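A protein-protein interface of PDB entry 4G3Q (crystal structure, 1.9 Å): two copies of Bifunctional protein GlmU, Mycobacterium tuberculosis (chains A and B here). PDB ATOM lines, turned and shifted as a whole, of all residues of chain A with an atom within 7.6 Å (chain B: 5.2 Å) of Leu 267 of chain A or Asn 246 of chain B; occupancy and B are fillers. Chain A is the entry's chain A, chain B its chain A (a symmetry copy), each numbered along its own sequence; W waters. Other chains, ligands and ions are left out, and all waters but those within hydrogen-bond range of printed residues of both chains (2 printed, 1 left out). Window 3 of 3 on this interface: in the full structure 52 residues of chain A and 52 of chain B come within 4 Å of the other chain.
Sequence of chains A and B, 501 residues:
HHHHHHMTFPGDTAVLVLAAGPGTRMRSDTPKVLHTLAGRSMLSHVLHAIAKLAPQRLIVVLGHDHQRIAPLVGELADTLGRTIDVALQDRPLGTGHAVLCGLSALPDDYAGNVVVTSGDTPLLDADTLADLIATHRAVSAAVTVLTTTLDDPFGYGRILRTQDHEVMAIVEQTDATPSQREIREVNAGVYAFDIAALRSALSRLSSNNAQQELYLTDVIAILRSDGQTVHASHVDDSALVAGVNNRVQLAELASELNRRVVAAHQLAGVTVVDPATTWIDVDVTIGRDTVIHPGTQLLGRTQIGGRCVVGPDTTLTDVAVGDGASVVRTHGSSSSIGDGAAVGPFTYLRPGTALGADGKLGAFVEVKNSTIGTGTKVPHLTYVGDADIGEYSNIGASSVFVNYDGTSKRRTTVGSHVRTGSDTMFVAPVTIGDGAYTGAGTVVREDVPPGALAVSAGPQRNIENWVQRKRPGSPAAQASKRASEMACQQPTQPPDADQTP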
ATOM      1  N   ARG A 260     -31.479  -2.631 -17.279  1.00  0.00           N
ATOM      2  CA  ARG A 260     -31.459  -1.349 -18.005  1.00  0.00           C
ATOM      3  C   ARG A 260     -30.747  -0.250 -17.212  1.00  0.00           C
ATOM      4  O   ARG A 260     -30.004   0.524 -17.793  1.00  0.00           O
ATOM      5  CB  ARG A 260     -32.898  -0.904 -18.312  1.00  0.00           C
ATOM      6  CG  ARG A 260     -33.485  -1.887 -19.301  1.00  0.00           C
ATOM      7  CD  ARG A 260     -34.930  -1.568 -19.701  1.00  0.00           C
ATOM      8  NE  ARG A 260     -35.374  -2.602 -20.650  1.00  0.00           N
ATOM      9  CZ  ARG A 260     -36.245  -2.344 -21.652  1.00  0.00           C
ATOM     10  NH1 ARG A 260     -36.745  -1.102 -21.824  1.00  0.00           N
ATOM     11  NH2 ARG A 260     -36.581  -3.325 -22.486  1.00  0.00           N
ATOM     12  N   VAL A 261     -30.979  -0.192 -15.914  1.00  0.00           N
ATOM     13  CA  VAL A 261     -30.300   0.764 -15.065  1.00  0.00           C
ATOM     14  C   VAL A 261     -28.765   0.479 -15.048  1.00  0.00           C
ATOM     15  O   VAL A 261     -27.911   1.390 -15.187  1.00  0.00           O
ATOM     16  CB  VAL A 261     -30.855   0.712 -13.601  1.00  0.00           C
ATOM     17  CG1 VAL A 261     -29.926   1.597 -12.612  1.00  0.00           C
ATOM     18  CG2 VAL A 261     -32.421   1.156 -13.534  1.00  0.00           C
ATOM     19  N   VAL A 262     -28.416  -0.772 -14.864  1.00  0.00           N
ATOM     20  CA  VAL A 262     -27.018  -1.130 -14.831  1.00  0.00           C
ATOM     21  C   VAL A 262     -26.384  -0.748 -16.174  1.00  0.00           C
ATOM     22  O   VAL A 262     -25.265  -0.224 -16.204  1.00  0.00           O
ATOM     23  CB  VAL A 262     -26.845  -2.669 -14.620  1.00  0.00           C
ATOM     24  CG1 VAL A 262     -25.392  -3.129 -14.886  1.00  0.00           C
ATOM     25  CG2 VAL A 262     -27.161  -2.996 -13.125  1.00  0.00           C
ATOM     26  N   ALA A 263     -27.075  -1.077 -17.268  1.00  0.00           N
ATOM     27  CA  ALA A 263     -26.498  -0.825 -18.594  1.00  0.00           C
ATOM     28  C   ALA A 263     -26.206   0.646 -18.802  1.00  0.00           C
ATOM     29  O   ALA A 263     -25.156   0.965 -19.416  1.00  0.00           O
ATOM     30  CB  ALA A 263     -27.373  -1.366 -19.797  1.00  0.00           C
ATOM     31  N   ALA A 264     -27.117   1.498 -18.362  1.00  0.00           N
ATOM     32  CA  ALA A 264     -26.921   2.947 -18.411  1.00  0.00           C
ATOM     33  C   ALA A 264     -25.684   3.393 -17.660  1.00  0.00           C
ATOM     34  O   ALA A 264     -24.899   4.192 -18.195  1.00  0.00           O
ATOM     35  CB  ALA A 264     -28.153   3.736 -17.895  1.00  0.00           C
ATOM     36  N   HIS A 265     -25.441   2.852 -16.477  1.00  0.00           N
ATOM     37  CA  HIS A 265     -24.197   3.106 -15.789  1.00  0.00           C
ATOM     38  C   HIS A 265     -22.931   2.612 -16.525  1.00  0.00           C
ATOM     39  O   HIS A 265     -21.911   3.354 -16.540  1.00  0.00           O
ATOM     40  CB  HIS A 265     -24.240   2.543 -14.333  1.00  0.00           C
ATOM     41  CG  HIS A 265     -25.185   3.281 -13.447  1.00  0.00           C
ATOM     42  ND1 HIS A 265     -24.956   4.572 -13.038  1.00  0.00           N
ATOM     43  CD2 HIS A 265     -26.385   2.921 -12.925  1.00  0.00           C
ATOM     44  CE1 HIS A 265     -25.943   4.960 -12.244  1.00  0.00           C
ATOM     45  NE2 HIS A 265     -26.837   3.977 -12.192  1.00  0.00           N
ATOM     46  N   GLN A 266     -22.954   1.374 -17.051  1.00  0.00           N
ATOM     47  CA  GLN A 266     -21.846   0.853 -17.839  1.00  0.00           C
ATOM     48  C   GLN A 266     -21.522   1.734 -19.037  1.00  0.00           C
ATOM     49  O   GLN A 266     -20.340   2.056 -19.256  1.00  0.00           O
ATOM     50  CB  GLN A 266     -22.157  -0.559 -18.371  1.00  0.00           C
ATOM     51  CG  GLN A 266     -22.243  -1.551 -17.191  1.00  0.00           C
ATOM     52  CD  GLN A 266     -22.790  -2.855 -17.718  1.00  0.00           C
ATOM     53  OE1 GLN A 266     -23.889  -2.876 -18.307  1.00  0.00           O
ATOM     54  NE2 GLN A 266     -22.088  -3.938 -17.493  1.00  0.00           N
ATOM     55  N   LEU A 267     -22.570   2.188 -19.750  1.00  0.00           N
ATOM     56  CA  LEU A 267     -22.318   3.042 -20.953  1.00  0.00           C
ATOM     57  C   LEU A 267     -21.795   4.407 -20.522  1.00  0.00           C
ATOM     58  O   LEU A 267     -21.049   5.033 -21.301  1.00  0.00           O
ATOM     59  CB  LEU A 267     -23.555   3.214 -21.804  1.00  0.00           C
ATOM     60  CG  LEU A 267     -23.984   1.877 -22.451  1.00  0.00           C
ATOM     61  CD1 LEU A 267     -25.247   2.132 -23.212  1.00  0.00           C
ATOM     62  CD2 LEU A 267     -22.890   1.311 -23.404  1.00  0.00           C
ATOM     63  N   ALA A 268     -22.073   4.795 -19.273  1.00  0.00           N
ATOM     64  CA  ALA A 268     -21.549   6.056 -18.745  1.00  0.00           C
ATOM     65  C   ALA A 268     -20.171   5.949 -18.079  1.00  0.00           C
ATOM     66  O   ALA A 268     -19.624   6.922 -17.553  1.00  0.00           O
ATOM     67  CB  ALA A 268     -22.567   6.779 -17.819  1.00  0.00           C
ATOM     68  N   GLY A 269     -19.577   4.786 -18.096  1.00  0.00           N
ATOM     69  CA  GLY A 269     -18.274   4.699 -17.513  1.00  0.00           C
ATOM     70  C   GLY A 269     -18.116   3.906 -16.234  1.00  0.00           C
ATOM     71  O   GLY A 269     -17.024   3.971 -15.601  1.00  0.00           O
ATOM     72  N   VAL A 270     -19.101   3.071 -15.890  1.00  0.00           N
ATOM     73  CA  VAL A 270     -18.956   2.330 -14.610  1.00  0.00           C
ATOM     74  C   VAL A 270     -18.745   0.841 -14.977  1.00  0.00           C
ATOM     75  O   VAL A 270     -19.539   0.277 -15.728  1.00  0.00           O
ATOM     76  CB  VAL A 270     -20.263   2.410 -13.731  1.00  0.00           C
ATOM     77  CG1 VAL A 270     -20.125   1.534 -12.450  1.00  0.00           C
ATOM     78  CG2 VAL A 270     -20.588   3.882 -13.401  1.00  0.00           C
ATOM     79  N   THR A 271     -17.683   0.237 -14.483  1.00  0.00           N
ATOM     80  CA  THR A 271     -17.517  -1.200 -14.601  1.00  0.00           C
ATOM     81  C   THR A 271     -18.422  -1.951 -13.638  1.00  0.00           C
ATOM     82  O   THR A 271     -18.321  -1.740 -12.404  1.00  0.00           O
ATOM     83  CB  THR A 271     -16.043  -1.573 -14.330  1.00  0.00           C
ATOM     84  OG1 THR A 271     -15.265  -1.127 -15.443  1.00  0.00           O
ATOM     85  CG2 THR A 271     -15.885  -3.125 -14.286  1.00  0.00           C
ATOM     86  N   ARG B  25     -15.703   4.776 -26.388  1.00  0.00           N
ATOM     87  CA  ARG B  25     -16.930   4.166 -25.900  1.00  0.00           C
ATOM     88  C   ARG B  25     -16.844   3.431 -24.547  1.00  0.00           C
ATOM     89  O   ARG B  25     -17.878   3.190 -23.906  1.00  0.00           O
ATOM     90  CB  ARG B  25     -17.589   3.330 -26.974  1.00  0.00           C
ATOM     91  CG  ARG B  25     -18.228   4.195 -28.117  1.00  0.00           C
ATOM     92  CD  ARG B  25     -18.619   3.228 -29.313  1.00  0.00           C
ATOM     93  NE  ARG B  25     -17.392   2.706 -29.973  1.00  0.00           N
ATOM     94  CZ  ARG B  25     -17.406   1.898 -31.032  1.00  0.00           C
ATOM     95  NH1 ARG B  25     -18.580   1.414 -31.479  1.00  0.00           N
ATOM     96  NH2 ARG B  25     -16.265   1.511 -31.641  1.00  0.00           N
ATOM     97  N   MET B  26     -15.628   3.066 -24.125  1.00  0.00           N
ATOM     98  CA  MET B  26     -15.445   2.516 -22.761  1.00  0.00           C
ATOM     99  C   MET B  26     -15.694   3.579 -21.693  1.00  0.00           C
ATOM    100  O   MET B  26     -15.968   3.219 -20.542  1.00  0.00           O
ATOM    101  CB  MET B  26     -14.040   1.980 -22.581  1.00  0.00           C
ATOM    102  CG  MET B  26     -13.663   0.843 -23.556  1.00  0.00           C
ATOM    103  SD  MET B  26     -14.683  -0.683 -23.375  1.00  0.00           S
ATOM    104  CE  MET B  26     -13.949  -1.313 -21.853  1.00  0.00           C
ATOM    105  N   ARG B  27     -15.561   4.891 -22.046  1.00  0.00           N
ATOM    106  CA  ARG B  27     -15.681   6.021 -21.046  1.00  0.00           C
ATOM    107  C   ARG B  27     -14.814   5.744 -19.847  1.00  0.00           C
ATOM    108  O   ARG B  27     -15.285   5.752 -18.699  1.00  0.00           O
ATOM    109  CB  ARG B  27     -17.125   6.259 -20.599  1.00  0.00           C
ATOM    110  CG  ARG B  27     -18.131   6.383 -21.718  1.00  0.00           C
ATOM    111  CD  ARG B  27     -18.396   7.809 -22.122  1.00  0.00           C
ATOM    112  NE  ARG B  27     -18.773   7.732 -23.525  1.00  0.00           N
ATOM    113  CZ  ARG B  27     -18.396   8.576 -24.491  1.00  0.00           C
ATOM    114  NH1 ARG B  27     -17.664   9.675 -24.224  1.00  0.00           N
ATOM    115  NH2 ARG B  27     -18.767   8.311 -25.747  1.00  0.00           N
ATOM    116  N   VAL B 244     -15.546  -6.100 -28.148  1.00  0.00           N
ATOM    117  CA  VAL B 244     -15.869  -5.343 -26.929  1.00  0.00           C
ATOM    118  C   VAL B 244     -15.553  -3.919 -27.211  1.00  0.00           C
ATOM    119  O   VAL B 244     -14.362  -3.547 -27.243  1.00  0.00           O
ATOM    120  CB  VAL B 244     -15.029  -5.848 -25.666  1.00  0.00           C
ATOM    121  CG1 VAL B 244     -15.238  -4.963 -24.449  1.00  0.00           C
ATOM    122  CG2 VAL B 244     -15.360  -7.424 -25.315  1.00  0.00           C
ATOM    123  N   ASN B 245     -16.582  -3.116 -27.461  1.00  0.00           N
ATOM    124  CA  ASN B 245     -16.395  -1.654 -27.613  1.00  0.00           C
ATOM    125  C   ASN B 245     -16.857  -0.844 -26.428  1.00  0.00           C
ATOM    126  O   ASN B 245     -16.603   0.375 -26.349  1.00  0.00           O
ATOM    127  CB  ASN B 245     -17.107  -1.097 -28.866  1.00  0.00           C
ATOM    128  CG  ASN B 245     -16.477  -1.576 -30.148  1.00  0.00           C
ATOM    129  OD1 ASN B 245     -15.295  -1.919 -30.142  1.00  0.00           O
ATOM    130  ND2 ASN B 245     -17.282  -1.691 -31.231  1.00  0.00           N
ATOM    131  N   ASN B 246     -17.573  -1.471 -25.487  1.00  0.00           N
ATOM    132  CA  ASN B 246     -18.092  -0.658 -24.336  1.00  0.00           C
ATOM    133  C   ASN B 246     -18.201  -1.650 -23.145  1.00  0.00           C
ATOM    134  O   ASN B 246     -17.974  -2.854 -23.333  1.00  0.00           O
ATOM    135  CB  ASN B 246     -19.436   0.062 -24.643  1.00  0.00           C
ATOM    136  CG  ASN B 246     -20.559  -0.933 -24.970  1.00  0.00           C
ATOM    137  OD1 ASN B 246     -20.660  -1.974 -24.298  1.00  0.00           O
ATOM    138  ND2 ASN B 246     -21.362  -0.659 -26.032  1.00  0.00           N
ATOM    139  N   ARG B 247     -18.550  -1.149 -21.970  1.00  0.00           N
ATOM    140  CA  ARG B 247     -18.553  -1.943 -20.771  1.00  0.00           C
ATOM    141  C   ARG B 247     -19.722  -2.903 -20.689  1.00  0.00           C
ATOM    142  O   ARG B 247     -19.701  -3.830 -19.842  1.00  0.00           O
ATOM    143  CB  ARG B 247     -18.597  -0.986 -19.566  1.00  0.00           C
ATOM    144  CG  ARG B 247     -17.171  -0.322 -19.319  1.00  0.00           C
ATOM    145  CD  ARG B 247     -17.052   0.271 -17.927  1.00  0.00           C
ATOM    146  NE  ARG B 247     -16.311   1.430 -18.036  1.00  0.00           N
ATOM    147  CZ  ARG B 247     -15.351   1.959 -17.299  1.00  0.00           C
ATOM    148  NH1 ARG B 247     -14.766   1.518 -16.200  1.00  0.00           N
ATOM    149  NH2 ARG B 247     -15.039   3.123 -17.758  1.00  0.00           N
ATOM    150  N   VAL B 248     -20.800  -2.598 -21.389  1.00  0.00           N
ATOM    151  CA  VAL B 248     -21.907  -3.576 -21.523  1.00  0.00           C
ATOM    152  C   VAL B 248     -21.418  -4.844 -22.238  1.00  0.00           C
ATOM    153  O   VAL B 248     -21.614  -6.008 -21.766  1.00  0.00           O
ATOM    154  CB  VAL B 248     -23.137  -3.042 -22.343  1.00  0.00           C
ATOM    155  CG1 VAL B 248     -24.235  -4.113 -22.496  1.00  0.00           C
ATOM    156  CG2 VAL B 248     -23.708  -1.737 -21.715  1.00  0.00           C
ATOM    157  N   GLN B 249     -20.750  -4.646 -23.375  1.00  0.00           N
ATOM    158  CA  GLN B 249     -20.194  -5.829 -24.114  1.00  0.00           C
ATOM    159  C   GLN B 249     -19.098  -6.526 -23.331  1.00  0.00           C
ATOM    160  O   GLN B 249     -18.951  -7.749 -23.404  1.00  0.00           O
ATOM    161  CB  GLN B 249     -19.610  -5.378 -25.467  1.00  0.00           C
ATOM    162  CG  GLN B 249     -20.781  -4.894 -26.386  1.00  0.00           C
ATOM    163  CD  GLN B 249     -20.350  -4.548 -27.811  1.00  0.00           C
ATOM    164  OE1 GLN B 249     -19.235  -4.115 -28.031  1.00  0.00           O
ATOM    165  NE2 GLN B 249     -21.222  -4.838 -28.782  1.00  0.00           N
ATOM    166  N   LEU B 250     -18.300  -5.770 -22.603  1.00  0.00           N
ATOM    167  CA  LEU B 250     -17.234  -6.373 -21.828  1.00  0.00           C
ATOM    168  C   LEU B 250     -17.858  -7.362 -20.772  1.00  0.00           C
ATOM    169  O   LEU B 250     -17.370  -8.550 -20.674  1.00  0.00           O
ATOM    170  CB  LEU B 250     -16.390  -5.270 -21.130  1.00  0.00           C
ATOM    171  CG  LEU B 250     -15.302  -5.777 -20.142  1.00  0.00           C
ATOM    172  CD1 LEU B 250     -14.307  -6.744 -20.783  1.00  0.00           C
ATOM    173  CD2 LEU B 250     -14.572  -4.635 -19.471  1.00  0.00           C
HETATM  174  O   HOH W   1     -19.114  -3.583 -16.901  1.00  0.00           O
HETATM  175  O   HOH W   2     -20.308   4.332 -24.094  1.00  0.00           O
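O of Arg 247 of chain B lies within hydrogen-bond range of NE2 of Gln 266 of chain A, 3.4 Å away.
The guanidinium group (NH2) of Arg 247 of chain B is in hydrogen-bond range of the backbone carbonyl oxygen (O) of Gly 269 of chain A, at 3.1 Å.
The side-chain hydroxyl (OG1) of Thr 271 of chain A is in hydrogen-bond range of the guanidinium group (NH1) of Arg 247 of chain B (2.8 Å).
OD1 of Asn 246 of chain B sits at hydrogen-bond distance from N of Gln 249 of chain B.
OD1 of Asn 246 of chain B lies within hydrogen-bond range of N of Val 248 of chain B (3.0 Å).
The backbone carbonyl oxygen (O) of Met 26 of chain B is in hydrogen-bond range of the guanidinium group (NH2) of Arg 247 of chain B (2.9 Å).
The backbone NH of Asn 246 of chain B lies close to the side-chain sulfur of Met 26 of chain B, 3.7 Å away.
O of His 265 of chain A sits at hydrogen-bond distance from N of Val 270 of chain A.
NH2 of Arg 247 of chain B sits at hydrogen-bond distance from O of Arg 27 of chain B.
Ala 263 of chain A touches Val 248 of chain B.
Val 248 of chain B touches Gln 266 of chain A (CG2 to OE1, 3.6 Å).
Leu 267 of chain A touches Arg 27 of chain B (O to CG, 3.2 Å).
Leu 267 of chain A touches Asn 246 of chain B.
CD2 of Leu 267 of chain A touches CG2 of Val 248 of chain B, 3.6 Å away.
C of Ala 268 of chain A touches CB of Arg 27 of chain B, 3.97 Å away.
Arg 27 of chain B touches Gly 269 of chain A.
Val 270 of chain A touches Arg 247 of chain B (O to CD, 3.3 Å).
Leu 267 of chain A touches three residues of chain B.
Of the printed residues of chain B, Thr 271 of chain A touches Arg 247 (2.8 Å).
Arg 25 of chain B touches none of the printed residues of chain A.
Printed residues of chain A within 4 Å of Arg 27 of chain B: Leu 267, Ala 268 and Gly 269.
Asn 246 of chain B touches just one residue of chain A: Leu 267.
Of the printed residues of chain A, Arg 247 of chain B touches Gln 266, Gly 269, Val 270 and Thr 271.
The nearest residue of chain B that does not touch Leu 267 of chain A is Arg 25 of chain B (4.5 Å).
The nearest residue of chain A that does not touch Asn 246 of chain B is Gln 266 of chain A (5.8 Å).
The nearest printed residue of chain A that does not touch Arg 27 of chain B is Val 270 of chain A (5.4 Å).
Of the 12 printed residues of chain A, 7 touch a printed residue of chain B.
Hydrophobic or aromatic side chains of chain A that line the printed part of chain B: Leu 267.
Along chain B the printed residues that touch a printed residue of chain A span positions 27 to 248.
No position is printed for both chains.
Of the 11 pairs that touch across the chains among the printed residues, none has its exchanged pair printed and touching as well.
Water W2 bridges the backbone carbonyl oxygen of Arg 25 of chain B and the backbone carbonyl oxygen of Leu 267 of chain A.
Water W1 bridges O of Arg 247 of chain B (3.0 Å) and NE2 of Gln 266 of chain A (3.1 Å).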
